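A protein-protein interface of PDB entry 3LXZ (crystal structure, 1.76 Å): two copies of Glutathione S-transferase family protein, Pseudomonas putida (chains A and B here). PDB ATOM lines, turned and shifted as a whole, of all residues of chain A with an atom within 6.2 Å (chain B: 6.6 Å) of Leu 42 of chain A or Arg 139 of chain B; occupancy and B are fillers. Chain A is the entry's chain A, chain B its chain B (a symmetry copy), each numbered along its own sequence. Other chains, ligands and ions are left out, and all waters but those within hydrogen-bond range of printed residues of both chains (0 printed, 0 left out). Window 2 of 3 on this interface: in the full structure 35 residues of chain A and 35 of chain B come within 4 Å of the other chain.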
ATOM      1  N   PHE A  33     -24.793  14.560  29.375  1.00  0.00           N
ATOM      2  CA  PHE A  33     -24.166  13.420  28.685  1.00  0.00           C
ATOM      3  C   PHE A  33     -23.247  14.043  27.630  1.00  0.00           C
ATOM      4  O   PHE A  33     -23.692  14.841  26.810  1.00  0.00           O
ATOM      5  CB  PHE A  33     -25.223  12.531  28.009  1.00  0.00           C
ATOM      6  CG  PHE A  33     -24.640  11.439  27.122  1.00  0.00           C
ATOM      7  CD1 PHE A  33     -24.070  10.275  27.660  1.00  0.00           C
ATOM      8  CD2 PHE A  33     -24.688  11.576  25.755  1.00  0.00           C
ATOM      9  CE1 PHE A  33     -23.538   9.260  26.815  1.00  0.00           C
ATOM     10  CE2 PHE A  33     -24.162  10.580  24.915  1.00  0.00           C
ATOM     11  CZ  PHE A  33     -23.583   9.422  25.460  1.00  0.00           C
ATOM     12  N   GLY A  36     -18.563  10.770  23.632  1.00  0.00           N
ATOM     13  CA  GLY A  36     -17.166  10.351  23.639  1.00  0.00           C
ATOM     14  C   GLY A  36     -17.036   8.825  23.591  1.00  0.00           C
ATOM     15  O   GLY A  36     -18.022   8.069  23.451  1.00  0.00           O
ATOM     16  N   GLN A  37     -15.798   8.370  23.718  1.00  0.00           N
ATOM     17  CA  GLN A  37     -15.429   6.979  23.417  1.00  0.00           C
ATOM     18  C   GLN A  37     -15.355   6.012  24.607  1.00  0.00           C
ATOM     19  O   GLN A  37     -14.951   4.848  24.442  1.00  0.00           O
ATOM     20  CB  GLN A  37     -14.089   6.965  22.652  1.00  0.00           C
ATOM     21  CG  GLN A  37     -14.063   7.863  21.417  1.00  0.00           C
ATOM     22  CD  GLN A  37     -15.193   7.517  20.457  1.00  0.00           C
ATOM     23  OE1 GLN A  37     -15.451   6.338  20.194  1.00  0.00           O
ATOM     24  NE2 GLN A  37     -15.890   8.547  19.954  1.00  0.00           N
ATOM     25  N   ALA A  38     -15.734   6.461  25.804  1.00  0.00           N
ATOM     26  CA  ALA A  38     -15.783   5.540  26.938  1.00  0.00           C
ATOM     27  C   ALA A  38     -16.796   4.425  26.653  1.00  0.00           C
ATOM     28  O   ALA A  38     -17.842   4.676  26.024  1.00  0.00           O
ATOM     29  CB  ALA A  38     -16.142   6.272  28.235  1.00  0.00           C
ATOM     30  N   PRO A  39     -16.491   3.185  27.100  1.00  0.00           N
ATOM     31  CA  PRO A  39     -17.376   2.058  26.806  1.00  0.00           C
ATOM     32  C   PRO A  39     -18.804   2.270  27.274  1.00  0.00           C
ATOM     33  O   PRO A  39     -19.743   1.850  26.582  1.00  0.00           O
ATOM     34  CB  PRO A  39     -16.722   0.880  27.550  1.00  0.00           C
ATOM     35  CG  PRO A  39     -15.256   1.245  27.589  1.00  0.00           C
ATOM     36  CD  PRO A  39     -15.225   2.744  27.731  1.00  0.00           C
ATOM     37  N   GLN A  40     -18.995   2.913  28.422  1.00  0.00           N
ATOM     38  CA  GLN A  40     -20.360   3.169  28.879  1.00  0.00           C
ATOM     39  C   GLN A  40     -21.106   4.164  27.962  1.00  0.00           C
ATOM     40  O   GLN A  40     -22.313   4.031  27.753  1.00  0.00           O
ATOM     41  CB  GLN A  40     -20.392   3.662  30.342  1.00  0.00           C
ATOM     42  CG  GLN A  40     -20.182   2.556  31.385  1.00  0.00           C
ATOM     43  CD  GLN A  40     -20.565   2.999  32.812  1.00  0.00           C
ATOM     44  OE1 GLN A  40     -21.607   2.590  33.347  1.00  0.00           O
ATOM     45  NE2 GLN A  40     -19.726   3.846  33.423  1.00  0.00           N
ATOM     46  N   ALA A  41     -20.371   5.143  27.433  1.00  0.00           N
ATOM     47  CA  ALA A  41     -20.931   6.193  26.579  1.00  0.00           C
ATOM     48  C   ALA A  41     -21.304   5.599  25.223  1.00  0.00           C
ATOM     49  O   ALA A  41     -22.344   5.939  24.671  1.00  0.00           O
ATOM     50  CB  ALA A  41     -19.948   7.311  26.414  1.00  0.00           C
ATOM     51  N   LEU A  42     -20.488   4.661  24.728  1.00  0.00           N
ATOM     52  CA  LEU A  42     -20.752   3.988  23.437  1.00  0.00           C
ATOM     53  C   LEU A  42     -21.988   3.108  23.488  1.00  0.00           C
ATOM     54  O   LEU A  42     -22.606   2.817  22.453  1.00  0.00           O
ATOM     55  CB  LEU A  42     -19.544   3.170  22.957  1.00  0.00           C
ATOM     56  CG  LEU A  42     -18.354   4.040  22.545  1.00  0.00           C
ATOM     57  CD1 LEU A  42     -17.087   3.218  22.115  1.00  0.00           C
ATOM     58  CD2 LEU A  42     -18.711   5.080  21.491  1.00  0.00           C
ATOM     59  N   GLU A  43     -22.348   2.661  24.688  1.00  0.00           N
ATOM     60  CA  GLU A  43     -23.593   1.923  24.847  1.00  0.00           C
ATOM     61  C   GLU A  43     -24.843   2.783  24.666  1.00  0.00           C
ATOM     62  O   GLU A  43     -25.915   2.275  24.335  1.00  0.00           O
ATOM     63  CB  GLU A  43     -23.632   1.226  26.210  1.00  0.00           C
ATOM     64  CG  GLU A  43     -22.866  -0.088  26.249  1.00  0.00           C
ATOM     65  CD  GLU A  43     -23.396  -0.947  27.366  1.00  0.00           C
ATOM     66  OE1 GLU A  43     -24.066  -1.967  27.075  1.00  0.00           O
ATOM     67  OE2 GLU A  43     -23.203  -0.541  28.535  1.00  0.00           O
ATOM     68  N   VAL A  44     -24.711   4.084  24.885  1.00  0.00           N
ATOM     69  CA  VAL A  44     -25.832   4.999  24.655  1.00  0.00           C
ATOM     70  C   VAL A  44     -25.819   5.538  23.215  1.00  0.00           C
ATOM     71  O   VAL A  44     -26.853   5.571  22.521  1.00  0.00           O
ATOM     72  CB  VAL A  44     -25.779   6.216  25.606  1.00  0.00           C
ATOM     73  CG1 VAL A  44     -27.002   7.156  25.342  1.00  0.00           C
ATOM     74  CG2 VAL A  44     -25.666   5.747  27.091  1.00  0.00           C
ATOM     75  N   SER A  45     -24.638   5.973  22.785  1.00  0.00           N
ATOM     76  CA  SER A  45     -24.471   6.593  21.481  1.00  0.00           C
ATOM     77  C   SER A  45     -23.364   5.879  20.723  1.00  0.00           C
ATOM     78  O   SER A  45     -22.225   5.986  21.123  1.00  0.00           O
ATOM     79  CB  SER A  45     -24.079   8.044  21.648  1.00  0.00           C
ATOM     80  OG  SER A  45     -24.252   8.713  20.414  1.00  0.00           O
ATOM     81  N   PRO A  46     -23.708   5.161  19.636  1.00  0.00           N
ATOM     82  CA  PRO A  46     -22.749   4.156  19.146  1.00  0.00           C
ATOM     83  C   PRO A  46     -21.482   4.649  18.482  1.00  0.00           C
ATOM     84  O   PRO A  46     -20.598   3.855  18.308  1.00  0.00           O
ATOM     85  CB  PRO A  46     -23.532   3.332  18.133  1.00  0.00           C
ATOM     86  CG  PRO A  46     -24.957   3.896  18.082  1.00  0.00           C
ATOM     87  CD  PRO A  46     -25.086   4.955  19.126  1.00  0.00           C
ATOM     88  N   ARG A  47     -21.449   5.910  18.064  1.00  0.00           N
ATOM     89  CA  ARG A  47     -20.209   6.553  17.600  1.00  0.00           C
ATOM     90  C   ARG A  47     -19.712   7.621  18.589  1.00  0.00           C
ATOM     91  O   ARG A  47     -18.684   8.275  18.359  1.00  0.00           O
ATOM     92  CB  ARG A  47     -20.427   7.154  16.192  1.00  0.00           C
ATOM     93  CG  ARG A  47     -19.196   7.792  15.537  1.00  0.00           C
ATOM     94  CD  ARG A  47     -18.106   6.768  15.219  1.00  0.00           C
ATOM     95  NE  ARG A  47     -16.951   7.414  14.590  1.00  0.00           N
ATOM     96  CZ  ARG A  47     -15.941   7.956  15.263  1.00  0.00           C
ATOM     97  NH1 ARG A  47     -15.929   7.887  16.578  1.00  0.00           N
ATOM     98  NH2 ARG A  47     -14.936   8.547  14.613  1.00  0.00           N
ATOM     99  N   GLY A  48     -20.433   7.784  19.694  1.00  0.00           N
ATOM    100  CA  GLY A  48     -19.996   8.689  20.758  1.00  0.00           C
ATOM    101  C   GLY A  48     -20.462  10.117  20.506  1.00  0.00           C
ATOM    102  O   GLY A  48     -19.962  11.058  21.117  1.00  0.00           O
ATOM    103  N   LYS A  49     -21.409  10.277  19.588  1.00  0.00           N
ATOM    104  CA  LYS A  49     -21.907  11.608  19.233  1.00  0.00           C
ATOM    105  C   LYS A  49     -23.008  12.046  20.168  1.00  0.00           C
ATOM    106  O   LYS A  49     -23.646  11.258  20.808  1.00  0.00           O
ATOM    107  CB  LYS A  49     -22.487  11.637  17.799  1.00  0.00           C
ATOM    108  CG  LYS A  49     -21.461  11.354  16.662  1.00  0.00           C
ATOM    109  CD  LYS A  49     -20.190  12.184  16.776  1.00  0.00           C
ATOM    110  CE  LYS A  49     -19.170  11.638  15.817  1.00  0.00           C
ATOM    111  NZ  LYS A  49     -17.882  12.390  15.744  1.00  0.00           N
ATOM    112  N   ALA B 132     -13.100   3.221  13.918  1.00  0.00           N
ATOM    113  CA  ALA B 132     -14.230   3.617  14.747  1.00  0.00           C
ATOM    114  C   ALA B 132     -15.602   3.378  14.035  1.00  0.00           C
ATOM    115  O   ALA B 132     -16.588   2.922  14.665  1.00  0.00           O
ATOM    116  CB  ALA B 132     -14.089   5.074  15.171  1.00  0.00           C
ATOM    117  N   PHE B 134     -16.289   1.106  11.658  1.00  0.00           N
ATOM    118  CA  PHE B 134     -16.583  -0.332  11.671  1.00  0.00           C
ATOM    119  C   PHE B 134     -17.010  -0.875  13.037  1.00  0.00           C
ATOM    120  O   PHE B 134     -17.911  -1.726  13.122  1.00  0.00           O
ATOM    121  CB  PHE B 134     -15.437  -1.160  11.069  1.00  0.00           C
ATOM    122  CG  PHE B 134     -15.444  -1.189   9.578  1.00  0.00           C
ATOM    123  CD1 PHE B 134     -16.256  -2.086   8.889  1.00  0.00           C
ATOM    124  CD2 PHE B 134     -14.623  -0.324   8.843  1.00  0.00           C
ATOM    125  CE1 PHE B 134     -16.243  -2.151   7.508  1.00  0.00           C
ATOM    126  CE2 PHE B 134     -14.643  -0.354   7.429  1.00  0.00           C
ATOM    127  CZ  PHE B 134     -15.437  -1.269   6.774  1.00  0.00           C
ATOM    128  N   ALA B 135     -16.388  -0.353  14.098  1.00  0.00           N
ATOM    129  CA  ALA B 135     -16.800  -0.712  15.442  1.00  0.00           C
ATOM    130  C   ALA B 135     -18.224  -0.246  15.724  1.00  0.00           C
ATOM    131  O   ALA B 135     -19.011  -0.965  16.354  1.00  0.00           O
ATOM    132  CB  ALA B 135     -15.819  -0.136  16.432  1.00  0.00           C
ATOM    133  N   THR B 136     -18.566   0.947  15.253  1.00  0.00           N
ATOM    134  CA  THR B 136     -19.927   1.459  15.418  1.00  0.00           C
ATOM    135  C   THR B 136     -20.937   0.610  14.706  1.00  0.00           C
ATOM    136  O   THR B 136     -21.973   0.275  15.287  1.00  0.00           O
ATOM    137  CB  THR B 136     -20.034   2.907  14.908  1.00  0.00           C
ATOM    138  OG1 THR B 136     -19.274   3.725  15.775  1.00  0.00           O
ATOM    139  CG2 THR B 136     -21.493   3.375  14.925  1.00  0.00           C
ATOM    140  N   LEU B 137     -20.661   0.240  13.457  1.00  0.00           N
ATOM    141  CA  LEU B 137     -21.525  -0.704  12.719  1.00  0.00           C
ATOM    142  C   LEU B 137     -21.698  -2.055  13.454  1.00  0.00           C
ATOM    143  O   LEU B 137     -22.810  -2.609  13.522  1.00  0.00           O
ATOM    144  CB  LEU B 137     -20.970  -0.914  11.299  1.00  0.00           C
ATOM    145  CG  LEU B 137     -21.845  -1.709  10.302  1.00  0.00           C
ATOM    146  CD1 LEU B 137     -23.266  -1.158  10.156  1.00  0.00           C
ATOM    147  CD2 LEU B 137     -21.157  -1.821   8.937  1.00  0.00           C
ATOM    148  N   LYS B 138     -20.610  -2.563  14.029  1.00  0.00           N
ATOM    149  CA  LYS B 138     -20.672  -3.858  14.701  1.00  0.00           C
ATOM    150  C   LYS B 138     -21.537  -3.790  15.935  1.00  0.00           C
ATOM    151  O   LYS B 138     -22.291  -4.723  16.237  1.00  0.00           O
ATOM    152  CB  LYS B 138     -19.286  -4.356  15.106  1.00  0.00           C
ATOM    153  CG  LYS B 138     -19.329  -5.776  15.640  1.00  0.00           C
ATOM    154  CD  LYS B 138     -17.933  -6.240  16.044  1.00  0.00           C
ATOM    155  CE  LYS B 138     -16.995  -6.240  14.862  1.00  0.00           C
ATOM    156  NZ  LYS B 138     -16.008  -7.360  14.987  1.00  0.00           N
ATOM    157  N   ARG B 139     -21.423  -2.694  16.671  1.00  0.00           N
ATOM    158  CA  ARG B 139     -22.179  -2.585  17.898  1.00  0.00           C
ATOM    159  C   ARG B 139     -23.668  -2.276  17.641  1.00  0.00           C
ATOM    160  O   ARG B 139     -24.530  -2.744  18.390  1.00  0.00           O
ATOM    161  CB  ARG B 139     -21.493  -1.639  18.928  1.00  0.00           C
ATOM    162  CG  ARG B 139     -21.793  -0.147  18.854  1.00  0.00           C
ATOM    163  CD  ARG B 139     -21.151   0.589  20.110  1.00  0.00           C
ATOM    164  NE  ARG B 139     -19.770   0.167  20.364  1.00  0.00           N
ATOM    165  CZ  ARG B 139     -18.681   0.689  19.793  1.00  0.00           C
ATOM    166  NH1 ARG B 139     -18.800   1.712  18.944  1.00  0.00           N
ATOM    167  NH2 ARG B 139     -17.461   0.189  20.081  1.00  0.00           N
ATOM    168  N   ASN B 140     -23.966  -1.504  16.597  1.00  0.00           N
ATOM    169  CA  ASN B 140     -25.327  -1.010  16.379  1.00  0.00           C
ATOM    170  C   ASN B 140     -26.158  -1.824  15.406  1.00  0.00           C
ATOM    171  O   ASN B 140     -27.392  -1.793  15.483  1.00  0.00           O
ATOM    172  CB  ASN B 140     -25.317   0.483  15.956  1.00  0.00           C
ATOM    173  CG  ASN B 140     -26.642   1.194  16.243  1.00  0.00           C
ATOM    174  OD1 ASN B 140     -27.287   0.949  17.252  1.00  0.00           O
ATOM    175  ND2 ASN B 140     -27.021   2.111  15.374  1.00  0.00           N
ATOM    176  N   GLY B 141     -25.494  -2.533  14.495  1.00  0.00           N
ATOM    177  CA  GLY B 141     -26.139  -3.294  13.429  1.00  0.00           C
ATOM    178  C   GLY B 141     -26.693  -4.591  14.010  1.00  0.00           C
ATOM    179  O   GLY B 141     -26.166  -5.098  14.999  1.00  0.00           O
ATOM    180  N   ARG B 142     -27.749  -5.129  13.428  1.00  0.00           N
ATOM    181  CA  ARG B 142     -28.291  -6.375  13.927  1.00  0.00           C
ATOM    182  C   ARG B 142     -27.822  -7.564  13.105  1.00  0.00           C
ATOM    183  O   ARG B 142     -27.735  -8.694  13.614  1.00  0.00           O
ATOM    184  CB  ARG B 142     -29.804  -6.318  13.939  1.00  0.00           C
ATOM    185  CG  ARG B 142     -30.405  -5.404  15.029  1.00  0.00           C
ATOM    186  CD  ARG B 142     -31.834  -5.815  15.442  1.00  0.00           C
ATOM    187  NE  ARG B 142     -32.038  -7.281  15.487  1.00  0.00           N
ATOM    188  CZ  ARG B 142     -33.034  -7.943  14.876  1.00  0.00           C
ATOM    189  NH1 ARG B 142     -33.974  -7.292  14.190  1.00  0.00           N
ATOM    190  NH2 ARG B 142     -33.102  -9.266  14.972  1.00  0.00           N
ATOM    191  N   PHE B 143     -27.548  -7.329  11.820  1.00  0.00           N
ATOM    192  CA  PHE B 143     -27.127  -8.415  10.914  1.00  0.00           C
ATOM    193  C   PHE B 143     -27.917  -9.704  11.100  1.00  0.00           C
ATOM    194  O   PHE B 143     -27.340 -10.756  11.445  1.00  0.00           O
ATOM    195  CB  PHE B 143     -25.628  -8.634  11.075  1.00  0.00           C
ATOM    196  CG  PHE B 143     -24.811  -7.450  10.640  1.00  0.00           C
ATOM    197  CD1 PHE B 143     -24.369  -6.512  11.573  1.00  0.00           C
ATOM    198  CD2 PHE B 143     -24.532  -7.258   9.289  1.00  0.00           C
ATOM    199  CE1 PHE B 143     -23.631  -5.384  11.159  1.00  0.00           C
ATOM    200  CE2 PHE B 143     -23.776  -6.144   8.848  1.00  0.00           C
ATOM    201  CZ  PHE B 143     -23.348  -5.206   9.790  1.00  0.00           C
ATOM    202  N   PHE B 182     -14.993  -9.364  11.031  1.00  0.00           N
ATOM    203  CA  PHE B 182     -16.404  -8.885  11.039  1.00  0.00           C
ATOM    204  C   PHE B 182     -17.260  -9.876  10.252  1.00  0.00           C
ATOM    205  O   PHE B 182     -17.751  -9.561   9.151  1.00  0.00           O
ATOM    206  CB  PHE B 182     -16.466  -7.511  10.380  1.00  0.00           C
ATOM    207  CG  PHE B 182     -17.674  -6.688  10.759  1.00  0.00           C
ATOM    208  CD1 PHE B 182     -18.804  -7.273  11.344  1.00  0.00           C
ATOM    209  CD2 PHE B 182     -17.679  -5.308  10.501  1.00  0.00           C
ATOM    210  CE1 PHE B 182     -19.912  -6.470  11.688  1.00  0.00           C
ATOM    211  CE2 PHE B 182     -18.778  -4.513  10.820  1.00  0.00           C
ATOM    212  CZ  PHE B 182     -19.892  -5.097  11.425  1.00  0.00           C
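Leu 42 of chain A touches Arg 139 of chain B (O to CD, 3.5 Å).
Asn 140 of chain B touches Pro 46 of chain A.
Arg 47 of chain A touches Ala 132 of chain B.
Thr 136 of chain B touches Arg 47 of chain A.
No position is printed for both chains.
Leu 42 of chain A touches just one residue of chain B: Arg 139 (3.5 Å).
Printed residues of chain B within 4 Å of Arg 47 of chain A: Ala 132 (3.4 Å) and Thr 136 (3.3 Å).
Printed residues of chain A within 4 Å of Thr 136 of chain B: Pro 46 and Arg 47.
Arg 139 of chain B touches just these residues of chain A: Leu 42 (3.5 Å) and Pro 46 (2.9 Å).
Gly 141 of chain B touches none of the printed residues of chain A.
The nearest residue of chain A that does not touch Arg 139 of chain B is Arg 47 of chain A (5.0 Å).
NE2 of Gln 37 of chain A lies within hydrogen-bond range of O of Arg 47 of chain A (3.2 Å).
The side-chain hydroxyl (OG1) of Thr 136 of chain B is in hydrogen-bond range of the backbone carbonyl oxygen (O) of Ala 132 of chain B, at 3.0 Å.
OG1 of Thr 136 of chain B sits at hydrogen-bond distance from O of Pro 46 of chain A, 2.9 Å away.
O of Pro 46 of chain A is in hydrogen-bond range of NH1 of Arg 139 of chain B.
Printed residues of chain B that touch a printed residue of chain A: Ala 132, Thr 136, Arg 139 and Asn 140.
Hydrophobic or aromatic side chains of chain B within 4 Å of the printed part of chain A: Ala 132.
Along chain B the printed residues that touch a printed residue of chain A span positions 132 to 140.
Along chain A the printed residues that touch a printed residue of chain B span positions 42 to 47.
Among the printed residues, 6 pairs touch across the chains.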
